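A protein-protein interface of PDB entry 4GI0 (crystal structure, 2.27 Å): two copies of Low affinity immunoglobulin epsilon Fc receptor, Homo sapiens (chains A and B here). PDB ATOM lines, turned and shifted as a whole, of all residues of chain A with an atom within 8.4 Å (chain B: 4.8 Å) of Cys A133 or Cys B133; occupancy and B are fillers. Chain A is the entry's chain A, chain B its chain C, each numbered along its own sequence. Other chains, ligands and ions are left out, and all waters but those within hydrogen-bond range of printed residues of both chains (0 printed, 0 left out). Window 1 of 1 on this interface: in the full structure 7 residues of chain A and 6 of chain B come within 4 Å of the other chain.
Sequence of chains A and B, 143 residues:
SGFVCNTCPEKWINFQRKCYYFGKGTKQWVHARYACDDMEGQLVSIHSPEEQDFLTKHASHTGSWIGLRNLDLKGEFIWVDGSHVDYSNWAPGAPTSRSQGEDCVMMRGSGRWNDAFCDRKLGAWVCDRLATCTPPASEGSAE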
ATOM      1  N   GLY A   2     -16.702   9.507 -19.882  1.00  0.00           N
ATOM      2  CA  GLY A   2     -16.326   8.116 -20.283  1.00  0.00           C
ATOM      3  C   GLY A   2     -15.133   7.550 -19.521  1.00  0.00           C
ATOM      4  O   GLY A   2     -14.528   6.555 -19.939  1.00  0.00           O
ATOM      5  N   PHE A   3     -14.796   8.190 -18.402  1.00  0.00           N
ATOM      6  CA  PHE A   3     -13.708   7.752 -17.530  1.00  0.00           C
ATOM      7  C   PHE A   3     -14.312   6.913 -16.423  1.00  0.00           C
ATOM      8  O   PHE A   3     -15.161   7.403 -15.695  1.00  0.00           O
ATOM      9  CB  PHE A   3     -13.036   8.959 -16.875  1.00  0.00           C
ATOM     10  CG  PHE A   3     -12.110   9.706 -17.774  1.00  0.00           C
ATOM     11  CD1 PHE A   3     -12.593  10.683 -18.638  1.00  0.00           C
ATOM     12  CD2 PHE A   3     -10.730   9.435 -17.758  1.00  0.00           C
ATOM     13  CE1 PHE A   3     -11.723  11.371 -19.489  1.00  0.00           C
ATOM     14  CE2 PHE A   3      -9.858  10.132 -18.592  1.00  0.00           C
ATOM     15  CZ  PHE A   3     -10.356  11.098 -19.462  1.00  0.00           C
ATOM     16  N   VAL A   4     -13.886   5.658 -16.302  1.00  0.00           N
ATOM     17  CA  VAL A   4     -14.412   4.790 -15.257  1.00  0.00           C
ATOM     18  C   VAL A   4     -13.423   4.734 -14.094  1.00  0.00           C
ATOM     19  O   VAL A   4     -12.277   4.329 -14.263  1.00  0.00           O
ATOM     20  CB  VAL A   4     -14.859   3.390 -15.782  1.00  0.00           C
ATOM     21  CG1 VAL A   4     -15.393   3.482 -17.199  1.00  0.00           C
ATOM     22  CG2 VAL A   4     -13.737   2.390 -15.754  1.00  0.00           C
ATOM     23  N   CYS A   5     -13.861   5.179 -12.919  1.00  0.00           N
ATOM     24  CA  CYS A   5     -12.949   5.346 -11.793  1.00  0.00           C
ATOM     25  C   CYS A   5     -13.108   4.206 -10.804  1.00  0.00           C
ATOM     26  O   CYS A   5     -13.839   4.302  -9.822  1.00  0.00           O
ATOM     27  CB  CYS A   5     -13.121   6.717 -11.133  1.00  0.00           C
ATOM     28  SG  CYS A   5     -12.929   8.062 -12.324  1.00  0.00           S
ATOM     29  N   ASN A   6     -12.398   3.127 -11.085  1.00  0.00           N
ATOM     30  CA  ASN A   6     -12.467   1.918 -10.301  1.00  0.00           C
ATOM     31  C   ASN A   6     -11.115   1.279 -10.090  1.00  0.00           C
ATOM     32  O   ASN A   6     -11.045   0.149  -9.605  1.00  0.00           O
ATOM     33  CB  ASN A   6     -13.452   0.913 -10.921  1.00  0.00           C
ATOM     34  CG  ASN A   6     -13.172   0.627 -12.386  1.00  0.00           C
ATOM     35  OD1 ASN A   6     -12.025   0.678 -12.849  1.00  0.00           O
ATOM     36  ND2 ASN A   6     -14.234   0.299 -13.132  1.00  0.00           N
ATOM     37  N   THR A   7     -10.034   1.983 -10.431  1.00  0.00           N
ATOM     38  CA  THR A   7      -8.708   1.393 -10.271  1.00  0.00           C
ATOM     39  C   THR A   7      -8.200   1.656  -8.877  1.00  0.00           C
ATOM     40  O   THR A   7      -8.193   2.796  -8.417  1.00  0.00           O
ATOM     41  CB  THR A   7      -7.684   1.910 -11.295  1.00  0.00           C
ATOM     42  OG1 THR A   7      -8.254   1.871 -12.603  1.00  0.00           O
ATOM     43  CG2 THR A   7      -6.440   1.029 -11.291  1.00  0.00           C
ATOM     44  N   CYS A   8      -7.767   0.585  -8.221  1.00  0.00           N
ATOM     45  CA  CYS A   8      -7.187   0.649  -6.880  1.00  0.00           C
ATOM     46  C   CYS A   8      -5.870  -0.107  -6.905  1.00  0.00           C
ATOM     47  O   CYS A   8      -5.687  -0.990  -7.734  1.00  0.00           O
ATOM     48  CB  CYS A   8      -8.149   0.017  -5.872  1.00  0.00           C
ATOM     49  SG  CYS A   8      -9.709   0.947  -5.791  1.00  0.00           S
ATOM     50  N   GLN A  16     -17.293   3.060  -5.791  1.00  0.00           N
ATOM     51  CA  GLN A  16     -17.425   4.378  -6.408  1.00  0.00           C
ATOM     52  C   GLN A  16     -16.037   4.986  -6.657  1.00  0.00           C
ATOM     53  O   GLN A  16     -15.184   4.335  -7.271  1.00  0.00           O
ATOM     54  CB  GLN A  16     -18.388   5.296  -5.606  1.00  0.00           C
ATOM     55  CG  GLN A  16     -19.829   4.760  -5.646  1.00  0.00           C
ATOM     56  CD  GLN A  16     -20.888   5.548  -4.862  1.00  0.00           C
ATOM     57  OE1 GLN A  16     -22.053   5.144  -4.831  1.00  0.00           O
ATOM     58  NE2 GLN A  16     -20.508   6.658  -4.248  1.00  0.00           N
ATOM     59  N   ARG A  17     -15.776   6.193  -6.154  1.00  0.00           N
ATOM     60  CA  ARG A  17     -14.528   6.856  -6.462  1.00  0.00           C
ATOM     61  C   ARG A  17     -13.429   6.670  -5.450  1.00  0.00           C
ATOM     62  O   ARG A  17     -12.388   7.346  -5.523  1.00  0.00           O
ATOM     63  CB  ARG A  17     -14.754   8.331  -6.757  1.00  0.00           C
ATOM     64  CG  ARG A  17     -15.001   8.491  -8.228  1.00  0.00           C
ATOM     65  CD  ARG A  17     -15.110   9.923  -8.664  1.00  0.00           C
ATOM     66  NE  ARG A  17     -15.340   9.920 -10.100  1.00  0.00           N
ATOM     67  CZ  ARG A  17     -15.427  11.011 -10.839  1.00  0.00           C
ATOM     68  NH1 ARG A  17     -15.308  12.193 -10.261  1.00  0.00           N
ATOM     69  NH2 ARG A  17     -15.626  10.913 -12.151  1.00  0.00           N
ATOM     70  N   LEU A 130      -8.182   7.833  -2.788  1.00  0.00           N
ATOM     71  CA  LEU A 130      -8.904   8.110  -4.014  1.00  0.00           C
ATOM     72  C   LEU A 130      -8.577   7.075  -5.089  1.00  0.00           C
ATOM     73  O   LEU A 130      -7.407   6.723  -5.284  1.00  0.00           O
ATOM     74  CB  LEU A 130      -8.570   9.514  -4.518  1.00  0.00           C
ATOM     75  CG  LEU A 130      -9.077  10.720  -3.692  1.00  0.00           C
ATOM     76  CD1 LEU A 130      -8.631  12.019  -4.364  1.00  0.00           C
ATOM     77  CD2 LEU A 130     -10.589  10.696  -3.489  1.00  0.00           C
ATOM     78  N   ALA A 131      -9.620   6.606  -5.776  1.00  0.00           N
ATOM     79  CA  ALA A 131      -9.500   5.737  -6.932  1.00  0.00           C
ATOM     80  C   ALA A 131      -8.953   6.505  -8.121  1.00  0.00           C
ATOM     81  O   ALA A 131      -9.059   7.711  -8.174  1.00  0.00           O
ATOM     82  CB  ALA A 131     -10.846   5.130  -7.293  1.00  0.00           C
ATOM     83  N   THR A 132      -8.363   5.794  -9.076  1.00  0.00           N
ATOM     84  CA  THR A 132      -7.967   6.424 -10.329  1.00  0.00           C
ATOM     85  C   THR A 132      -8.764   5.856 -11.490  1.00  0.00           C
ATOM     86  O   THR A 132      -9.486   4.868 -11.327  1.00  0.00           O
ATOM     87  CB  THR A 132      -6.453   6.339 -10.609  1.00  0.00           C
ATOM     88  OG1 THR A 132      -6.034   4.969 -10.604  1.00  0.00           O
ATOM     89  CG2 THR A 132      -5.666   7.148  -9.600  1.00  0.00           C
ATOM     90  N   CYS A 133      -8.630   6.478 -12.659  1.00  0.00           N
ATOM     91  CA  CYS A 133      -9.581   6.253 -13.726  1.00  0.00           C
ATOM     92  C   CYS A 133      -8.983   5.706 -15.023  1.00  0.00           C
ATOM     93  O   CYS A 133      -7.892   6.088 -15.451  1.00  0.00           O
ATOM     94  CB  CYS A 133     -10.391   7.548 -13.975  1.00  0.00           C
ATOM     95  SG  CYS A 133     -10.917   8.368 -12.427  1.00  0.00           S
ATOM     96  N   THR A 134      -9.724   4.787 -15.622  1.00  0.00           N
ATOM     97  CA  THR A 134      -9.450   4.271 -16.932  1.00  0.00           C
ATOM     98  C   THR A 134      -9.921   5.298 -17.963  1.00  0.00           C
ATOM     99  O   THR A 134     -11.075   5.727 -17.908  1.00  0.00           O
ATOM    100  CB  THR A 134     -10.141   2.904 -17.106  1.00  0.00           C
ATOM    101  OG1 THR A 134      -9.252   1.881 -16.624  1.00  0.00           O
ATOM    102  CG2 THR A 134     -10.465   2.621 -18.575  1.00  0.00           C
ATOM    103  N   PRO A 135      -9.021   5.721 -18.879  1.00  0.00           N
ATOM    104  CA  PRO A 135      -9.389   6.661 -19.953  1.00  0.00           C
ATOM    105  C   PRO A 135     -10.386   6.037 -20.938  1.00  0.00           C
ATOM    106  O   PRO A 135     -10.364   4.819 -21.127  1.00  0.00           O
ATOM    107  CB  PRO A 135      -8.044   6.954 -20.652  1.00  0.00           C
ATOM    108  CG  PRO A 135      -7.181   5.774 -20.345  1.00  0.00           C
ATOM    109  CD  PRO A 135      -7.593   5.353 -18.946  1.00  0.00           C
ATOM    110  N   PRO A 136     -11.272   6.857 -21.548  1.00  0.00           N
ATOM    111  CA  PRO A 136     -12.251   6.283 -22.479  1.00  0.00           C
ATOM    112  C   PRO A 136     -11.560   5.676 -23.699  1.00  0.00           C
ATOM    113  O   PRO A 136     -10.662   6.295 -24.272  1.00  0.00           O
ATOM    114  CB  PRO A 136     -13.132   7.480 -22.867  1.00  0.00           C
ATOM    115  CG  PRO A 136     -12.308   8.683 -22.568  1.00  0.00           C
ATOM    116  CD  PRO A 136     -11.450   8.313 -21.392  1.00  0.00           C
ATOM    117  N   PHE B   3      -9.018  15.699 -15.717  1.00  0.00           N
ATOM    118  CA  PHE B   3      -8.484  14.304 -15.833  1.00  0.00           C
ATOM    119  C   PHE B   3      -7.048  14.308 -16.337  1.00  0.00           C
ATOM    120  O   PHE B   3      -6.801  14.680 -17.476  1.00  0.00           O
ATOM    121  CB  PHE B   3      -9.356  13.423 -16.758  1.00  0.00           C
ATOM    122  CG  PHE B   3     -10.632  12.925 -16.116  1.00  0.00           C
ATOM    123  CD1 PHE B   3     -10.612  11.865 -15.206  1.00  0.00           C
ATOM    124  CD2 PHE B   3     -11.860  13.506 -16.431  1.00  0.00           C
ATOM    125  CE1 PHE B   3     -11.785  11.411 -14.614  1.00  0.00           C
ATOM    126  CE2 PHE B   3     -13.042  13.054 -15.838  1.00  0.00           C
ATOM    127  CZ  PHE B   3     -13.004  12.006 -14.928  1.00  0.00           C
ATOM    128  N   VAL B   4      -6.110  13.915 -15.478  1.00  0.00           N
ATOM    129  CA  VAL B   4      -4.697  13.790 -15.856  1.00  0.00           C
ATOM    130  C   VAL B   4      -4.258  12.328 -15.704  1.00  0.00           C
ATOM    131  O   VAL B   4      -4.497  11.704 -14.661  1.00  0.00           O
ATOM    132  CB  VAL B   4      -3.761  14.815 -15.137  1.00  0.00           C
ATOM    133  CG1 VAL B   4      -4.479  15.557 -14.027  1.00  0.00           C
ATOM    134  CG2 VAL B   4      -2.459  14.181 -14.656  1.00  0.00           C
ATOM    135  N   CYS B   5      -3.648  11.786 -16.755  1.00  0.00           N
ATOM    136  CA  CYS B   5      -3.417  10.352 -16.818  1.00  0.00           C
ATOM    137  C   CYS B   5      -1.964   9.963 -16.659  1.00  0.00           C
ATOM    138  O   CYS B   5      -1.293   9.660 -17.647  1.00  0.00           O
ATOM    139  CB  CYS B   5      -3.991   9.778 -18.116  1.00  0.00           C
ATOM    140  SG  CYS B   5      -5.762  10.083 -18.317  1.00  0.00           S
ATOM    141  N   ASN B   6      -1.468   9.940 -15.430  1.00  0.00           N
ATOM    142  CA  ASN B   6      -0.096   9.479 -15.238  1.00  0.00           C
ATOM    143  C   ASN B   6       0.173   8.673 -13.981  1.00  0.00           C
ATOM    144  O   ASN B   6       1.235   8.780 -13.364  1.00  0.00           O
ATOM    145  CB  ASN B   6       0.913  10.612 -15.445  1.00  0.00           C
ATOM    146  CG  ASN B   6       0.748  11.731 -14.457  1.00  0.00           C
ATOM    147  OD1 ASN B   6       0.243  11.543 -13.347  1.00  0.00           O
ATOM    148  ND2 ASN B   6       1.188  12.918 -14.853  1.00  0.00           N
ATOM    149  N   ALA B 131      -1.584   4.226 -18.434  1.00  0.00           N
ATOM    150  CA  ALA B 131      -1.619   4.879 -17.129  1.00  0.00           C
ATOM    151  C   ALA B 131      -3.077   5.146 -16.732  1.00  0.00           C
ATOM    152  O   ALA B 131      -3.938   5.296 -17.594  1.00  0.00           O
ATOM    153  CB  ALA B 131      -0.819   6.184 -17.148  1.00  0.00           C
ATOM    154  N   THR B 132      -3.358   5.178 -15.437  1.00  0.00           N
ATOM    155  CA  THR B 132      -4.680   5.595 -14.990  1.00  0.00           C
ATOM    156  C   THR B 132      -4.683   7.089 -14.635  1.00  0.00           C
ATOM    157  O   THR B 132      -3.616   7.709 -14.539  1.00  0.00           O
ATOM    158  CB  THR B 132      -5.238   4.697 -13.868  1.00  0.00           C
ATOM    159  OG1 THR B 132      -4.349   4.705 -12.748  1.00  0.00           O
ATOM    160  CG2 THR B 132      -5.400   3.268 -14.372  1.00  0.00           C
ATOM    161  N   CYS B 133      -5.874   7.655 -14.459  1.00  0.00           N
ATOM    162  CA  CYS B 133      -6.039   9.105 -14.396  1.00  0.00           C
ATOM    163  C   CYS B 133      -6.632   9.620 -13.075  1.00  0.00           C
ATOM    164  O   CYS B 133      -7.504   8.993 -12.478  1.00  0.00           O
ATOM    165  CB  CYS B 133      -6.910   9.592 -15.563  1.00  0.00           C
ATOM    166  SG  CYS B 133      -6.667   8.699 -17.118  1.00  0.00           S
ATOM    167  N   THR B 134      -6.104  10.763 -12.650  1.00  0.00           N
ATOM    168  CA  THR B 134      -6.591  11.553 -11.545  1.00  0.00           C
ATOM    169  C   THR B 134      -7.871  12.297 -11.970  1.00  0.00           C
ATOM    170  O   THR B 134      -7.834  13.087 -12.920  1.00  0.00           O
ATOM    171  CB  THR B 134      -5.499  12.571 -11.122  1.00  0.00           C
ATOM    172  OG1 THR B 134      -4.489  11.903 -10.346  1.00  0.00           O
ATOM    173  CG2 THR B 134      -6.084  13.709 -10.301  1.00  0.00           C
ATOM    174  N   PRO B 135      -9.011  12.041 -11.288  1.00  0.00           N
ATOM    175  CA  PRO B 135     -10.217  12.804 -11.636  1.00  0.00           C
ATOM    176  C   PRO B 135     -10.083  14.283 -11.261  1.00  0.00           C
ATOM    177  O   PRO B 135      -9.363  14.600 -10.308  1.00  0.00           O
ATOM    178  CB  PRO B 135     -11.328  12.141 -10.799  1.00  0.00           C
ATOM    179  CG  PRO B 135     -10.622  11.376  -9.728  1.00  0.00           C
ATOM    180  CD  PRO B 135      -9.285  10.989 -10.292  1.00  0.00           C
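N of Cys B133 sits at hydrogen-bond distance from O of Cys A133, at 2.7 Å.
OG1 of Thr A132 is in hydrogen-bond range of OG1 of Thr B132 (2.7 Å).
The side-chain sulfur of Cys A5 sits at hydrogen-bond distance from the guanidinium group of Arg A17 (3.8 Å).
The backbone NH (N) of Ala A131 lies within hydrogen-bond range of the backbone carbonyl oxygen (O) of Arg A17 (2.9 Å).
N of Asn A6 lies within hydrogen-bond range of O of Thr A132, 3.4 Å away.
O of Thr A132 sits at hydrogen-bond distance from N of Thr A7.
The side-chain sulfur (SG) of Cys B5 is disulfide-bonded to the side-chain sulfur (SG) of Cys B133 (2.0 Å).
O of Thr B132 lies within hydrogen-bond range of N of Asn B6, 3.2 Å away.
Among the printed residues, pairs that only touch across the chains: Phe A3 with Phe B3 (3.5 Å), Phe A3 with Cys B133 (3.8 Å), Thr A7 with Thr B132 (3.6 Å), Arg A17 with Phe B3 (3.97 Å), Ala A131 with Pro B135 (3.9 Å), Thr A132 with Cys B133 (3.4 Å), Cys A133 with Phe B3 (3.8 Å), Cys A133 with Thr B132 (3.3 Å), Cys A133 with Pro B135 (3.8 Å), Pro A135 with Ala B131 (3.9 Å) and Pro A135 with Cys B133 (3.9 Å).
Asn A6 touches none of the printed residues of chain B.
Printed residues of chain B within 4 Å of Thr A7: Thr B132 (3.6 Å).
Cys A8 touches none of the printed residues of chain B.
Of the printed residues of chain B, Arg A17 touches Phe B3.
Of the printed residues of chain A, Phe B3 touches Phe A3 (3.5 Å), Arg A17 (3.97 Å) and Cys A133 (3.8 Å).
Of the printed residues of chain A, Ala B131 touches Pro A135.
Of the printed residues of chain A, Thr B132 touches Thr A7 (3.6 Å), Thr A132 (2.7 Å) and Cys A133 (3.3 Å).
Cys B133 touches just these residues of chain A: Phe A3, Thr A132, Cys A133 and Pro A135.
The nearest printed residue of chain B that does not touch Phe A3 is Cys B5 (4.1 Å).
Printed residues of chain A that touch a printed residue of chain B: Phe A3, Thr A7, Arg A17, Ala A131, Thr A132, Cys A133 and Pro A135.
Phe B3 touches its own counterpart, Phe A3.
Phe A3 touches Cys B133, and with the chains exchanged Cys A133 touches Phe B3.
Ala A131 touches Pro B135, and with the chains exchanged Pro A135 touches Ala B131.
Cys B133 touches its own counterpart, Cys A133.
Of the 13 pairs that touch across the chains among the printed residues, 11 have their exchanged pair printed and touching as well.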
